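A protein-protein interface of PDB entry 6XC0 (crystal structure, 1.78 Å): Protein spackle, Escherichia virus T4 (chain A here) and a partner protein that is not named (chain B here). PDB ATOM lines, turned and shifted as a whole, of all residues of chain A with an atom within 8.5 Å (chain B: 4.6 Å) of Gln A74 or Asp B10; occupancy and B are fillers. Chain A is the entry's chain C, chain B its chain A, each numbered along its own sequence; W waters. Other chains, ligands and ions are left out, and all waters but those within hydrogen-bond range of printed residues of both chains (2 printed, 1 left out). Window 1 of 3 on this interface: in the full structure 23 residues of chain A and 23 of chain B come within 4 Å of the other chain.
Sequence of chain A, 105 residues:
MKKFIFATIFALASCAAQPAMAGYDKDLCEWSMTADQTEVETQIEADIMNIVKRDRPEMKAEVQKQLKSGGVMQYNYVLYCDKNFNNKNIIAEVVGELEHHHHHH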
ATOM      1  N   GLN A  37     -35.127   9.515  14.174  1.00  0.00           N
ATOM      2  CA  GLN A  37     -34.481   8.595  15.105  1.00  0.00           C
ATOM      3  C   GLN A  37     -35.493   7.689  15.792  1.00  0.00           C
ATOM      4  O   GLN A  37     -35.273   6.477  15.916  1.00  0.00           O
ATOM      5  CB  GLN A  37     -33.689   9.378  16.144  1.00  0.00           C
ATOM      6  CG  GLN A  37     -33.087   8.509  17.268  1.00  0.00           C
ATOM      7  CD  GLN A  37     -32.260   9.342  18.230  1.00  0.00           C
ATOM      8  OE1 GLN A  37     -32.358  10.560  18.216  1.00  0.00           O
ATOM      9  NE2 GLN A  37     -31.440   8.689  19.075  1.00  0.00           N
ATOM     10  N   VAL A  40     -36.605   4.798  13.669  1.00  0.00           N
ATOM     11  CA  VAL A  40     -35.516   3.871  13.385  1.00  0.00           C
ATOM     12  C   VAL A  40     -35.166   3.045  14.605  1.00  0.00           C
ATOM     13  O   VAL A  40     -35.019   1.823  14.512  1.00  0.00           O
ATOM     14  CB  VAL A  40     -34.295   4.637  12.844  1.00  0.00           C
ATOM     15  CG1 VAL A  40     -33.113   3.682  12.617  1.00  0.00           C
ATOM     16  CG2 VAL A  40     -34.669   5.320  11.555  1.00  0.00           C
ATOM     17  N   GLU A  41     -35.103   3.676  15.774  1.00  0.00           N
ATOM     18  CA  GLU A  41     -34.789   2.916  16.969  1.00  0.00           C
ATOM     19  C   GLU A  41     -35.892   1.916  17.311  1.00  0.00           C
ATOM     20  O   GLU A  41     -35.596   0.819  17.793  1.00  0.00           O
ATOM     21  CB  GLU A  41     -34.520   3.871  18.111  1.00  0.00           C
ATOM     22  CG  GLU A  41     -33.230   4.632  17.765  1.00  0.00           C
ATOM     23  CD  GLU A  41     -32.638   5.424  18.898  1.00  0.00           C
ATOM     24  OE1 GLU A  41     -33.318   5.619  19.924  1.00  0.00           O
ATOM     25  OE2 GLU A  41     -31.469   5.870  18.729  1.00  0.00           O
ATOM     26  N   ILE A  44     -35.012  -0.989  14.973  1.00  0.00           N
ATOM     27  CA  ILE A  44     -33.811  -1.710  15.398  1.00  0.00           C
ATOM     28  C   ILE A  44     -34.098  -2.547  16.630  1.00  0.00           C
ATOM     29  O   ILE A  44     -33.725  -3.727  16.700  1.00  0.00           O
ATOM     30  CB  ILE A  44     -32.671  -0.725  15.680  1.00  0.00           C
ATOM     31  CG1 ILE A  44     -32.237  -0.104  14.370  1.00  0.00           C
ATOM     32  CG2 ILE A  44     -31.462  -1.466  16.303  1.00  0.00           C
ATOM     33  CD1 ILE A  44     -31.274   1.095  14.549  1.00  0.00           C
ATOM     34  N   ILE A  48     -33.780  -6.669  16.978  1.00  0.00           N
ATOM     35  CA  ILE A  48     -32.899  -7.292  17.969  1.00  0.00           C
ATOM     36  C   ILE A  48     -33.708  -8.158  18.927  1.00  0.00           C
ATOM     37  O   ILE A  48     -33.322  -9.293  19.245  1.00  0.00           O
ATOM     38  CB  ILE A  48     -32.093  -6.225  18.726  1.00  0.00           C
ATOM     39  CG1 ILE A  48     -31.145  -5.499  17.737  1.00  0.00           C
ATOM     40  CG2 ILE A  48     -31.306  -6.853  19.866  1.00  0.00           C
ATOM     41  CD1 ILE A  48     -30.287  -4.389  18.409  1.00  0.00           C
ATOM     42  N   GLN A  66     -28.396  -3.095  28.033  1.00  0.00           N
ATOM     43  CA  GLN A  66     -27.320  -2.553  27.188  1.00  0.00           C
ATOM     44  C   GLN A  66     -27.841  -1.527  26.186  1.00  0.00           C
ATOM     45  O   GLN A  66     -27.133  -0.569  25.830  1.00  0.00           O
ATOM     46  CB  GLN A  66     -26.619  -3.689  26.424  1.00  0.00           C
ATOM     47  CG  GLN A  66     -25.774  -4.624  27.318  1.00  0.00           C
ATOM     48  CD  GLN A  66     -24.661  -3.856  28.007  1.00  0.00           C
ATOM     49  OE1 GLN A  66     -23.997  -3.026  27.366  1.00  0.00           O
ATOM     50  NE2 GLN A  66     -24.412  -4.157  29.311  1.00  0.00           N
ATOM     51  N   LEU A  67     -29.031  -1.761  25.649  1.00  0.00           N
ATOM     52  CA  LEU A  67     -29.569  -0.804  24.703  1.00  0.00           C
ATOM     53  C   LEU A  67     -29.855   0.533  25.386  1.00  0.00           C
ATOM     54  O   LEU A  67     -29.628   1.607  24.795  1.00  0.00           O
ATOM     55  CB  LEU A  67     -30.826  -1.382  24.055  1.00  0.00           C
ATOM     56  CG  LEU A  67     -30.643  -2.641  23.193  1.00  0.00           C
ATOM     57  CD1 LEU A  67     -31.964  -3.002  22.520  1.00  0.00           C
ATOM     58  CD2 LEU A  67     -29.543  -2.419  22.163  1.00  0.00           C
ATOM     59  N   LYS A  68     -30.328   0.488  26.646  1.00  0.00           N
ATOM     60  CA  LYS A  68     -30.562   1.720  27.395  1.00  0.00           C
ATOM     61  C   LYS A  68     -29.257   2.414  27.744  1.00  0.00           C
ATOM     62  O   LYS A  68     -29.135   3.633  27.570  1.00  0.00           O
ATOM     63  CB  LYS A  68     -31.355   1.431  28.682  1.00  0.00           C
ATOM     64  CG  LYS A  68     -32.792   1.050  28.435  1.00  0.00           C
ATOM     65  CD  LYS A  68     -33.519   0.758  29.767  1.00  0.00           C
ATOM     66  CE  LYS A  68     -34.882   0.076  29.576  1.00  0.00           C
ATOM     67  NZ  LYS A  68     -35.911   0.967  28.957  1.00  0.00           N
ATOM     68  N   SER A  69     -28.257   1.663  28.217  1.00  0.00           N
ATOM     69  CA  SER A  69     -27.009   2.324  28.645  1.00  0.00           C
ATOM     70  C   SER A  69     -26.089   2.665  27.474  1.00  0.00           C
ATOM     71  O   SER A  69     -25.362   3.669  27.522  1.00  0.00           O
ATOM     72  CB  SER A  69     -26.234   1.436  29.625  1.00  0.00           C
ATOM     73  OG  SER A  69     -25.823   0.221  29.022  1.00  0.00           O
ATOM     74  N   GLY A  70     -26.098   1.858  26.425  1.00  0.00           N
ATOM     75  CA  GLY A  70     -25.155   2.034  25.348  1.00  0.00           C
ATOM     76  C   GLY A  70     -25.727   2.627  24.074  1.00  0.00           C
ATOM     77  O   GLY A  70     -24.962   3.041  23.205  1.00  0.00           O
ATOM     78  N   GLY A  71     -27.044   2.650  23.928  1.00  0.00           N
ATOM     79  CA  GLY A  71     -27.588   3.166  22.687  1.00  0.00           C
ATOM     80  C   GLY A  71     -28.131   2.070  21.784  1.00  0.00           C
ATOM     81  O   GLY A  71     -27.812   0.879  21.915  1.00  0.00           O
ATOM     82  N   VAL A  72     -28.975   2.515  20.838  1.00  0.00           N
ATOM     83  CA  VAL A  72     -29.633   1.663  19.861  1.00  0.00           C
ATOM     84  C   VAL A  72     -29.200   1.996  18.438  1.00  0.00           C
ATOM     85  O   VAL A  72     -29.048   1.097  17.603  1.00  0.00           O
ATOM     86  CB  VAL A  72     -31.174   1.813  19.990  1.00  0.00           C
ATOM     87  CG1 VAL A  72     -31.880   1.009  18.898  1.00  0.00           C
ATOM     88  CG2 VAL A  72     -31.617   1.369  21.332  1.00  0.00           C
ATOM     89  N   MET A  73     -29.027   3.290  18.139  1.00  0.00           N
ATOM     90  CA  MET A  73     -28.894   3.718  16.744  1.00  0.00           C
ATOM     91  C   MET A  73     -27.662   3.108  16.083  1.00  0.00           C
ATOM     92  O   MET A  73     -27.655   2.885  14.863  1.00  0.00           O
ATOM     93  CB  MET A  73     -28.821   5.241  16.678  1.00  0.00           C
ATOM     94  CG  MET A  73     -28.650   5.784  15.275  1.00  0.00           C
ATOM     95  SD  MET A  73     -30.074   5.408  14.221  1.00  0.00           S
ATOM     96  CE  MET A  73     -31.299   6.335  15.105  1.00  0.00           C
ATOM     97  N   GLN A  74     -26.614   2.826  16.862  1.00  0.00           N
ATOM     98  CA  GLN A  74     -25.382   2.445  16.207  1.00  0.00           C
ATOM     99  C   GLN A  74     -25.495   1.101  15.476  1.00  0.00           C
ATOM    100  O   GLN A  74     -24.654   0.806  14.637  1.00  0.00           O
ATOM    101  CB  GLN A  74     -24.230   2.419  17.223  1.00  0.00           C
ATOM    102  CG  GLN A  74     -24.414   1.331  18.353  1.00  0.00           C
ATOM    103  CD  GLN A  74     -25.011   1.909  19.600  1.00  0.00           C
ATOM    104  OE1 GLN A  74     -25.923   2.734  19.528  1.00  0.00           O
ATOM    105  NE2 GLN A  74     -24.486   1.485  20.787  1.00  0.00           N
ATOM    106  N   TYR A  75     -26.501   0.279  15.773  1.00  0.00           N
ATOM    107  CA  TYR A  75     -26.599  -1.022  15.143  1.00  0.00           C
ATOM    108  C   TYR A  75     -27.209  -0.951  13.743  1.00  0.00           C
ATOM    109  O   TYR A  75     -27.363  -2.012  13.106  1.00  0.00           O
ATOM    110  CB  TYR A  75     -27.435  -1.972  16.026  1.00  0.00           C
ATOM    111  CG  TYR A  75     -26.809  -2.076  17.380  1.00  0.00           C
ATOM    112  CD1 TYR A  75     -25.567  -2.682  17.520  1.00  0.00           C
ATOM    113  CD2 TYR A  75     -27.402  -1.528  18.494  1.00  0.00           C
ATOM    114  CE1 TYR A  75     -24.924  -2.766  18.779  1.00  0.00           C
ATOM    115  CE2 TYR A  75     -26.760  -1.597  19.763  1.00  0.00           C
ATOM    116  CZ  TYR A  75     -25.515  -2.204  19.879  1.00  0.00           C
ATOM    117  OH  TYR A  75     -24.884  -2.284  21.131  1.00  0.00           O
ATOM    118  N   ASN A  76     -27.560   0.250  13.263  1.00  0.00           N
ATOM    119  CA  ASN A  76     -28.203   0.306  11.955  1.00  0.00           C
ATOM    120  C   ASN A  76     -27.264  -0.247  10.886  1.00  0.00           C
ATOM    121  O   ASN A  76     -27.714  -0.914   9.945  1.00  0.00           O
ATOM    122  CB  ASN A  76     -28.675   1.732  11.617  1.00  0.00           C
ATOM    123  CG  ASN A  76     -27.546   2.643  11.064  1.00  0.00           C
ATOM    124  OD1 ASN A  76     -26.496   2.813  11.658  1.00  0.00           O
ATOM    125  ND2 ASN A  76     -27.793   3.223   9.901  1.00  0.00           N
ATOM    126  N   TYR A  77     -25.955   0.031  10.999  1.00  0.00           N
ATOM    127  CA  TYR A  77     -25.067  -0.350   9.914  1.00  0.00           C
ATOM    128  C   TYR A  77     -24.943  -1.874   9.812  1.00  0.00           C
ATOM    129  O   TYR A  77     -25.168  -2.455   8.738  1.00  0.00           O
ATOM    130  CB  TYR A  77     -23.692   0.298  10.080  1.00  0.00           C
ATOM    131  CG  TYR A  77     -22.876  -0.022   8.854  1.00  0.00           C
ATOM    132  CD1 TYR A  77     -23.063   0.709   7.702  1.00  0.00           C
ATOM    133  CD2 TYR A  77     -21.962  -1.076   8.829  1.00  0.00           C
ATOM    134  CE1 TYR A  77     -22.374   0.416   6.550  1.00  0.00           C
ATOM    135  CE2 TYR A  77     -21.244  -1.373   7.646  1.00  0.00           C
ATOM    136  CZ  TYR A  77     -21.468  -0.623   6.535  1.00  0.00           C
ATOM    137  OH  TYR A  77     -20.789  -0.877   5.366  1.00  0.00           O
ATOM    138  N   VAL A  78     -24.641  -2.559  10.928  1.00  0.00           N
ATOM    139  CA  VAL A  78     -24.454  -3.999  10.804  1.00  0.00           C
ATOM    140  C   VAL A  78     -25.768  -4.696  10.466  1.00  0.00           C
ATOM    141  O   VAL A  78     -25.753  -5.721   9.776  1.00  0.00           O
ATOM    142  CB  VAL A  78     -23.824  -4.626  12.071  1.00  0.00           C
ATOM    143  CG1 VAL A  78     -22.342  -4.281  12.128  1.00  0.00           C
ATOM    144  CG2 VAL A  78     -24.574  -4.166  13.328  1.00  0.00           C
ATOM    145  N   LEU A  79     -26.909  -4.175  10.941  1.00  0.00           N
ATOM    146  CA  LEU A  79     -28.173  -4.892  10.737  1.00  0.00           C
ATOM    147  C   LEU A  79     -28.699  -4.776   9.319  1.00  0.00           C
ATOM    148  O   LEU A  79     -29.343  -5.713   8.823  1.00  0.00           O
ATOM    149  CB  LEU A  79     -29.260  -4.381  11.681  1.00  0.00           C
ATOM    150  CG  LEU A  79     -29.281  -4.897  13.121  1.00  0.00           C
ATOM    151  CD1 LEU A  79     -30.448  -4.248  13.866  1.00  0.00           C
ATOM    152  CD2 LEU A  79     -29.416  -6.420  13.138  1.00  0.00           C
ATOM    153  N   TYR A  80     -28.552  -3.602   8.705  1.00  0.00           N
ATOM    154  CA  TYR A  80     -29.251  -3.310   7.465  1.00  0.00           C
ATOM    155  C   TYR A  80     -28.339  -2.917   6.311  1.00  0.00           C
ATOM    156  O   TYR A  80     -28.777  -2.968   5.150  1.00  0.00           O
ATOM    157  CB  TYR A  80     -30.241  -2.159   7.680  1.00  0.00           C
ATOM    158  CG  TYR A  80     -31.186  -2.356   8.814  1.00  0.00           C
ATOM    159  CD1 TYR A  80     -31.936  -3.520   8.933  1.00  0.00           C
ATOM    160  CD2 TYR A  80     -31.323  -1.373   9.793  1.00  0.00           C
ATOM    161  CE1 TYR A  80     -32.811  -3.697  10.030  1.00  0.00           C
ATOM    162  CE2 TYR A  80     -32.173  -1.548  10.877  1.00  0.00           C
ATOM    163  CZ  TYR A  80     -32.931  -2.694  10.982  1.00  0.00           C
ATOM    164  OH  TYR A  80     -33.780  -2.828  12.083  1.00  0.00           O
ATOM    165  N   ILE A  90     -26.260 -10.517  16.211  1.00  0.00           N
ATOM    166  CA  ILE A  90     -26.491  -9.227  16.832  1.00  0.00           C
ATOM    167  C   ILE A  90     -26.569  -9.358  18.355  1.00  0.00           C
ATOM    168  O   ILE A  90     -26.308  -8.382  19.065  1.00  0.00           O
ATOM    169  CB  ILE A  90     -27.767  -8.560  16.270  1.00  0.00           C
ATOM    170  CG1 ILE A  90     -27.747  -7.068  16.577  1.00  0.00           C
ATOM    171  CG2 ILE A  90     -29.047  -9.281  16.861  1.00  0.00           C
ATOM    172  CD1 ILE A  90     -26.678  -6.299  15.739  1.00  0.00           C
ATOM    173  N   GLU A  93     -23.167  -8.988  19.391  1.00  0.00           N
ATOM    174  CA  GLU A  93     -22.799  -7.610  19.093  1.00  0.00           C
ATOM    175  C   GLU A  93     -23.172  -6.662  20.235  1.00  0.00           C
ATOM    176  O   GLU A  93     -22.446  -5.708  20.514  1.00  0.00           O
ATOM    177  CB  GLU A  93     -23.487  -7.134  17.812  1.00  0.00           C
ATOM    178  CG  GLU A  93     -22.880  -5.812  17.314  1.00  0.00           C
ATOM    179  CD  GLU A  93     -21.533  -6.036  16.593  1.00  0.00           C
ATOM    180  OE1 GLU A  93     -21.108  -7.222  16.458  1.00  0.00           O
ATOM    181  OE2 GLU A  93     -20.892  -5.032  16.173  1.00  0.00           O
ATOM    182  N   VAL A  94     -24.312  -6.894  20.877  1.00  0.00           N
ATOM    183  CA  VAL A  94     -24.794  -6.019  21.948  1.00  0.00           C
ATOM    184  C   VAL A  94     -24.170  -6.398  23.289  1.00  0.00           C
ATOM    185  O   VAL A  94     -23.778  -5.523  24.068  1.00  0.00           O
ATOM    186  CB  VAL A  94     -26.334  -6.089  22.037  1.00  0.00           C
ATOM    187  CG1 VAL A  94     -26.838  -5.353  23.290  1.00  0.00           C
ATOM    188  CG2 VAL A  94     -26.968  -5.461  20.819  1.00  0.00           C
ATOM    189  N   MET B   6     -13.941  -0.217  11.055  1.00  0.00           N
ATOM    190  CA  MET B   6     -14.128  -0.546  12.475  1.00  0.00           C
ATOM    191  C   MET B   6     -15.156   0.387  13.133  1.00  0.00           C
ATOM    192  O   MET B   6     -16.081  -0.065  13.829  1.00  0.00           O
ATOM    193  CB  MET B   6     -12.764  -0.467  13.188  1.00  0.00           C
ATOM    194  CG  MET B   6     -12.797  -1.000  14.615  1.00  0.00           C
ATOM    195  SD  MET B   6     -11.308  -0.473  15.515  1.00  0.00           S
ATOM    196  CE  MET B   6     -11.195  -1.710  16.798  1.00  0.00           C
ATOM    197  N   LEU B   7     -15.024   1.699  12.922  1.00  0.00           N
ATOM    198  CA  LEU B   7     -15.921   2.623  13.603  1.00  0.00           C
ATOM    199  C   LEU B   7     -17.276   2.729  12.918  1.00  0.00           C
ATOM    200  O   LEU B   7     -18.274   3.008  13.600  1.00  0.00           O
ATOM    201  CB  LEU B   7     -15.244   4.013  13.782  1.00  0.00           C
ATOM    202  CG  LEU B   7     -14.153   3.979  14.881  1.00  0.00           C
ATOM    203  CD1 LEU B   7     -13.198   5.194  14.767  1.00  0.00           C
ATOM    204  CD2 LEU B   7     -14.679   3.923  16.355  1.00  0.00           C
ATOM    205  N   ARG B   8     -17.373   2.457  11.614  1.00  0.00           N
ATOM    206  CA  ARG B   8     -18.716   2.368  11.017  1.00  0.00           C
ATOM    207  C   ARG B   8     -19.527   1.268  11.712  1.00  0.00           C
ATOM    208  O   ARG B   8     -20.725   1.424  11.989  1.00  0.00           O
ATOM    209  CB  ARG B   8     -18.585   2.063   9.534  1.00  0.00           C
ATOM    210  CG  ARG B   8     -19.775   2.352   8.689  1.00  0.00           C
ATOM    211  CD  ARG B   8     -19.406   2.161   7.215  1.00  0.00           C
ATOM    212  NE  ARG B   8     -18.602   0.952   6.985  1.00  0.00           N
ATOM    213  CZ  ARG B   8     -18.086   0.605   5.806  1.00  0.00           C
ATOM    214  NH1 ARG B   8     -18.307   1.357   4.735  1.00  0.00           N
ATOM    215  NH2 ARG B   8     -17.363  -0.507   5.691  1.00  0.00           N
ATOM    216  N   ARG B   9     -18.868   0.156  11.988  1.00  0.00           N
ATOM    217  CA  ARG B   9     -19.483  -0.964  12.704  1.00  0.00           C
ATOM    218  C   ARG B   9     -19.906  -0.568  14.116  1.00  0.00           C
ATOM    219  O   ARG B   9     -21.036  -0.860  14.546  1.00  0.00           O
ATOM    220  CB  ARG B   9     -18.514  -2.136  12.766  1.00  0.00           C
ATOM    221  CG  ARG B   9     -19.092  -3.302  13.593  1.00  0.00           C
ATOM    222  CD  ARG B   9     -18.279  -4.511  13.428  1.00  0.00           C
ATOM    223  NE  ARG B   9     -18.778  -5.606  14.263  1.00  0.00           N
ATOM    224  CZ  ARG B   9     -18.354  -6.852  14.146  1.00  0.00           C
ATOM    225  NH1 ARG B   9     -17.480  -7.129  13.183  1.00  0.00           N
ATOM    226  NH2 ARG B   9     -18.849  -7.818  14.942  1.00  0.00           N
ATOM    227  N   ASP B  10     -19.008   0.063  14.875  1.00  0.00           N
ATOM    228  CA  ASP B  10     -19.318   0.308  16.289  1.00  0.00           C
ATOM    229  C   ASP B  10     -20.171   1.548  16.502  1.00  0.00           C
ATOM    230  O   ASP B  10     -20.903   1.600  17.491  1.00  0.00           O
ATOM    231  CB  ASP B  10     -18.028   0.448  17.151  1.00  0.00           C
ATOM    232  CG  ASP B  10     -17.273  -0.849  17.304  1.00  0.00           C
ATOM    233  OD1 ASP B  10     -17.894  -1.942  17.169  1.00  0.00           O
ATOM    234  OD2 ASP B  10     -16.044  -0.792  17.603  1.00  0.00           O
ATOM    235  N   GLU B  11     -20.122   2.548  15.592  1.00  0.00           N
ATOM    236  CA  GLU B  11     -20.843   3.810  15.745  1.00  0.00           C
ATOM    237  C   GLU B  11     -22.078   3.928  14.852  1.00  0.00           C
ATOM    238  O   GLU B  11     -22.926   4.797  15.110  1.00  0.00           O
ATOM    239  CB  GLU B  11     -19.926   5.015  15.409  1.00  0.00           C
ATOM    240  CG  GLU B  11     -18.622   5.052  16.277  1.00  0.00           C
ATOM    241  CD  GLU B  11     -18.830   5.754  17.616  1.00  0.00           C
ATOM    242  OE1 GLU B  11     -17.897   5.748  18.483  1.00  0.00           O
ATOM    243  OE2 GLU B  11     -19.942   6.312  17.805  1.00  0.00           O
ATOM    244  N   GLY B  12     -22.213   3.065  13.848  1.00  0.00           N
ATOM    245  CA  GLY B  12     -23.332   3.189  12.932  1.00  0.00           C
ATOM    246  C   GLY B  12     -23.074   4.294  11.933  1.00  0.00           C
ATOM    247  O   GLY B  12     -21.998   4.896  11.900  1.00  0.00           O
ATOM    248  N   ASN B 106     -10.095   3.260  19.004  1.00  0.00           N
ATOM    249  CA  ASN B 106     -11.528   3.034  19.061  1.00  0.00           C
ATOM    250  C   ASN B 106     -12.086   3.568  20.387  1.00  0.00           C
ATOM    251  O   ASN B 106     -13.086   4.298  20.413  1.00  0.00           O
ATOM    252  CB  ASN B 106     -11.781   1.534  18.866  1.00  0.00           C
ATOM    253  CG  ASN B 106     -13.245   1.201  18.783  1.00  0.00           C
ATOM    254  OD1 ASN B 106     -13.961   1.477  19.699  1.00  0.00           O
ATOM    255  ND2 ASN B 106     -13.682   0.591  17.684  1.00  0.00           N
ATOM    256  N   ARG B 150     -19.258  -3.565  22.638  1.00  0.00           N
ATOM    257  CA  ARG B 150     -18.120  -2.865  22.069  1.00  0.00           C
ATOM    258  C   ARG B 150     -16.887  -3.085  22.929  1.00  0.00           C
ATOM    259  O   ARG B 150     -15.814  -3.394  22.407  1.00  0.00           O
ATOM    260  CB  ARG B 150     -18.438  -1.388  21.925  1.00  0.00           C
ATOM    261  CG  ARG B 150     -17.328  -0.583  21.280  1.00  0.00           C
ATOM    262  CD  ARG B 150     -17.896   0.813  20.971  1.00  0.00           C
ATOM    263  NE  ARG B 150     -16.886   1.674  20.324  1.00  0.00           N
ATOM    264  CZ  ARG B 150     -17.170   2.900  19.882  1.00  0.00           C
ATOM    265  NH1 ARG B 150     -16.226   3.645  19.311  1.00  0.00           N
ATOM    266  NH2 ARG B 150     -18.387   3.419  20.071  1.00  0.00           N
ATOM    267  N   ARG B 153     -15.391  -6.553  22.179  1.00  0.00           N
ATOM    268  CA  ARG B 153     -14.611  -6.624  20.936  1.00  0.00           C
ATOM    269  C   ARG B 153     -13.284  -5.917  21.088  1.00  0.00           C
ATOM    270  O   ARG B 153     -12.268  -6.385  20.557  1.00  0.00           O
ATOM    271  CB  ARG B 153     -15.352  -5.965  19.756  1.00  0.00           C
ATOM    272  CG  ARG B 153     -16.631  -6.656  19.381  1.00  0.00           C
ATOM    273  CD  ARG B 153     -17.248  -6.005  18.090  1.00  0.00           C
ATOM    274  NE  ARG B 153     -17.909  -4.698  18.279  1.00  0.00           N
ATOM    275  CZ  ARG B 153     -19.101  -4.552  18.874  1.00  0.00           C
ATOM    276  NH1 ARG B 153     -19.728  -5.600  19.388  1.00  0.00           N
ATOM    277  NH2 ARG B 153     -19.660  -3.366  18.991  1.00  0.00           N
ATOM    278  N   TYR B 166     -13.329  -8.439  15.185  1.00  0.00           N
ATOM    279  CA  TYR B 166     -14.059  -7.670  14.177  1.00  0.00           C
ATOM    280  C   TYR B 166     -14.192  -8.436  12.865  1.00  0.00           C
ATOM    281  O   TYR B 166     -14.428  -7.830  11.812  1.00  0.00           O
ATOM    282  CB  TYR B 166     -13.372  -6.329  13.923  1.00  0.00           C
ATOM    283  CG  TYR B 166     -13.687  -5.349  15.012  1.00  0.00           C
ATOM    284  CD1 TYR B 166     -13.023  -5.416  16.223  1.00  0.00           C
ATOM    285  CD2 TYR B 166     -14.664  -4.394  14.851  1.00  0.00           C
ATOM    286  CE1 TYR B 166     -13.305  -4.567  17.219  1.00  0.00           C
ATOM    287  CE2 TYR B 166     -14.954  -3.490  15.866  1.00  0.00           C
ATOM    288  CZ  TYR B 166     -14.285  -3.601  17.059  1.00  0.00           C
ATOM    289  OH  TYR B 166     -14.528  -2.769  18.124  1.00  0.00           O
HETATM  290  O   HOH W   1     -22.096  -2.548  16.593  1.00  0.00           O
HETATM  291  O   HOH W   2     -23.493  -0.973  13.072  1.00  0.00           O
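The backbone carbonyl oxygen (O) of Tyr B166 sits at hydrogen-bond distance from the guanidinium group (NH1) of Arg B9 (3.4 Å).
The side-chain carboxylate (OD2) of Asp B10 is in salt-bridge range of the guanidinium group (NE) of Arg B150.
The side-chain hydroxyl (OH) of Tyr B166 is in hydrogen-bond range of the side-chain carboxylate (OD2) of Asp B10, 2.5 Å away.
The backbone carbonyl oxygen (O) of Gly A70 is in hydrogen-bond range of the side-chain amide nitrogen (NE2) of Gln A74 (2.9 Å).
The side-chain amide oxygen (OE1) of Gln A74 is in hydrogen-bond range of the backbone NH (N) of Val A72 (3.3 Å).
O of Met A73 lies close to OD1 of Asn A76.
Of the printed residues of chain B, Gln A74 touches Arg B9, Asp B10, Glu B11 and Gly B12.
Asp B10 touches just one residue of chain A: Gln A74 (3.4 Å).
Printed residues of chain A within 4 Å of Arg B9: Gln A74 (3.98 Å), Val A78 (3.7 Å) and Glu A93 (2.8 Å).
Of the printed residues of chain B, Tyr A77 touches Arg B8 (3.1 Å).
Of the printed residues of chain A, Glu B11 touches Gln A74.
The nearest printed residue of chain B that does not touch Gln A74 is Arg B8 (4.8 Å).
The nearest residue of chain A that does not touch Asp B10 is Glu A93 (4.4 Å).
The nearest printed residue of chain B that does not touch Tyr A77 is Gly B12 (4.1 Å).
Gln A74 touches Arg B9 (O to O, 3.98 Å).
O of Asp B10 touches CB of Gln A74 (3.4 Å).
Gln A74 touches Glu B11 (CB to O, 3.4 Å).
Asn A76 touches Gly B12 (OD1 to CA, 3.4 Å).
Val A78 touches Arg B9 (CG1 to CG, 3.7 Å).
Of the 23 printed residues of chain A, 5 touch a printed residue of chain B.
Hydrophobic or aromatic side chains of chain A that line the printed part of chain B: Tyr A77 and Val A78.
Printed residues of chain B that touch a printed residue of chain A: Arg B8, Arg B9, Asp B10, Glu B11, Gly B12 and Arg B153.
Among the printed residues, 9 pairs touch across the chains.
The guanidinium group (NE) of Arg B8 sits close to the side-chain hydroxyl (OH) of Tyr A77, at 3.3 Å.
NH2 of Arg B9 lies within salt-bridge range of OE1 of Glu A93.
The backbone NH of Gly B12 lies close to the backbone carbonyl oxygen of Gln A74 (3.4 Å).
The side-chain carboxylate (OE2) of Glu A93 is in salt-bridge range of the guanidinium group (NH1) of Arg B153 (3.5 Å).
Water W2 lies within hydrogen-bond range of O of Gln A74, O of Arg B9, N of Val A78 and N of Tyr A77.
Water W1 bridges OE2 of Glu A93 (2.8 Å) and O of Arg B9 (2.9 Å).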
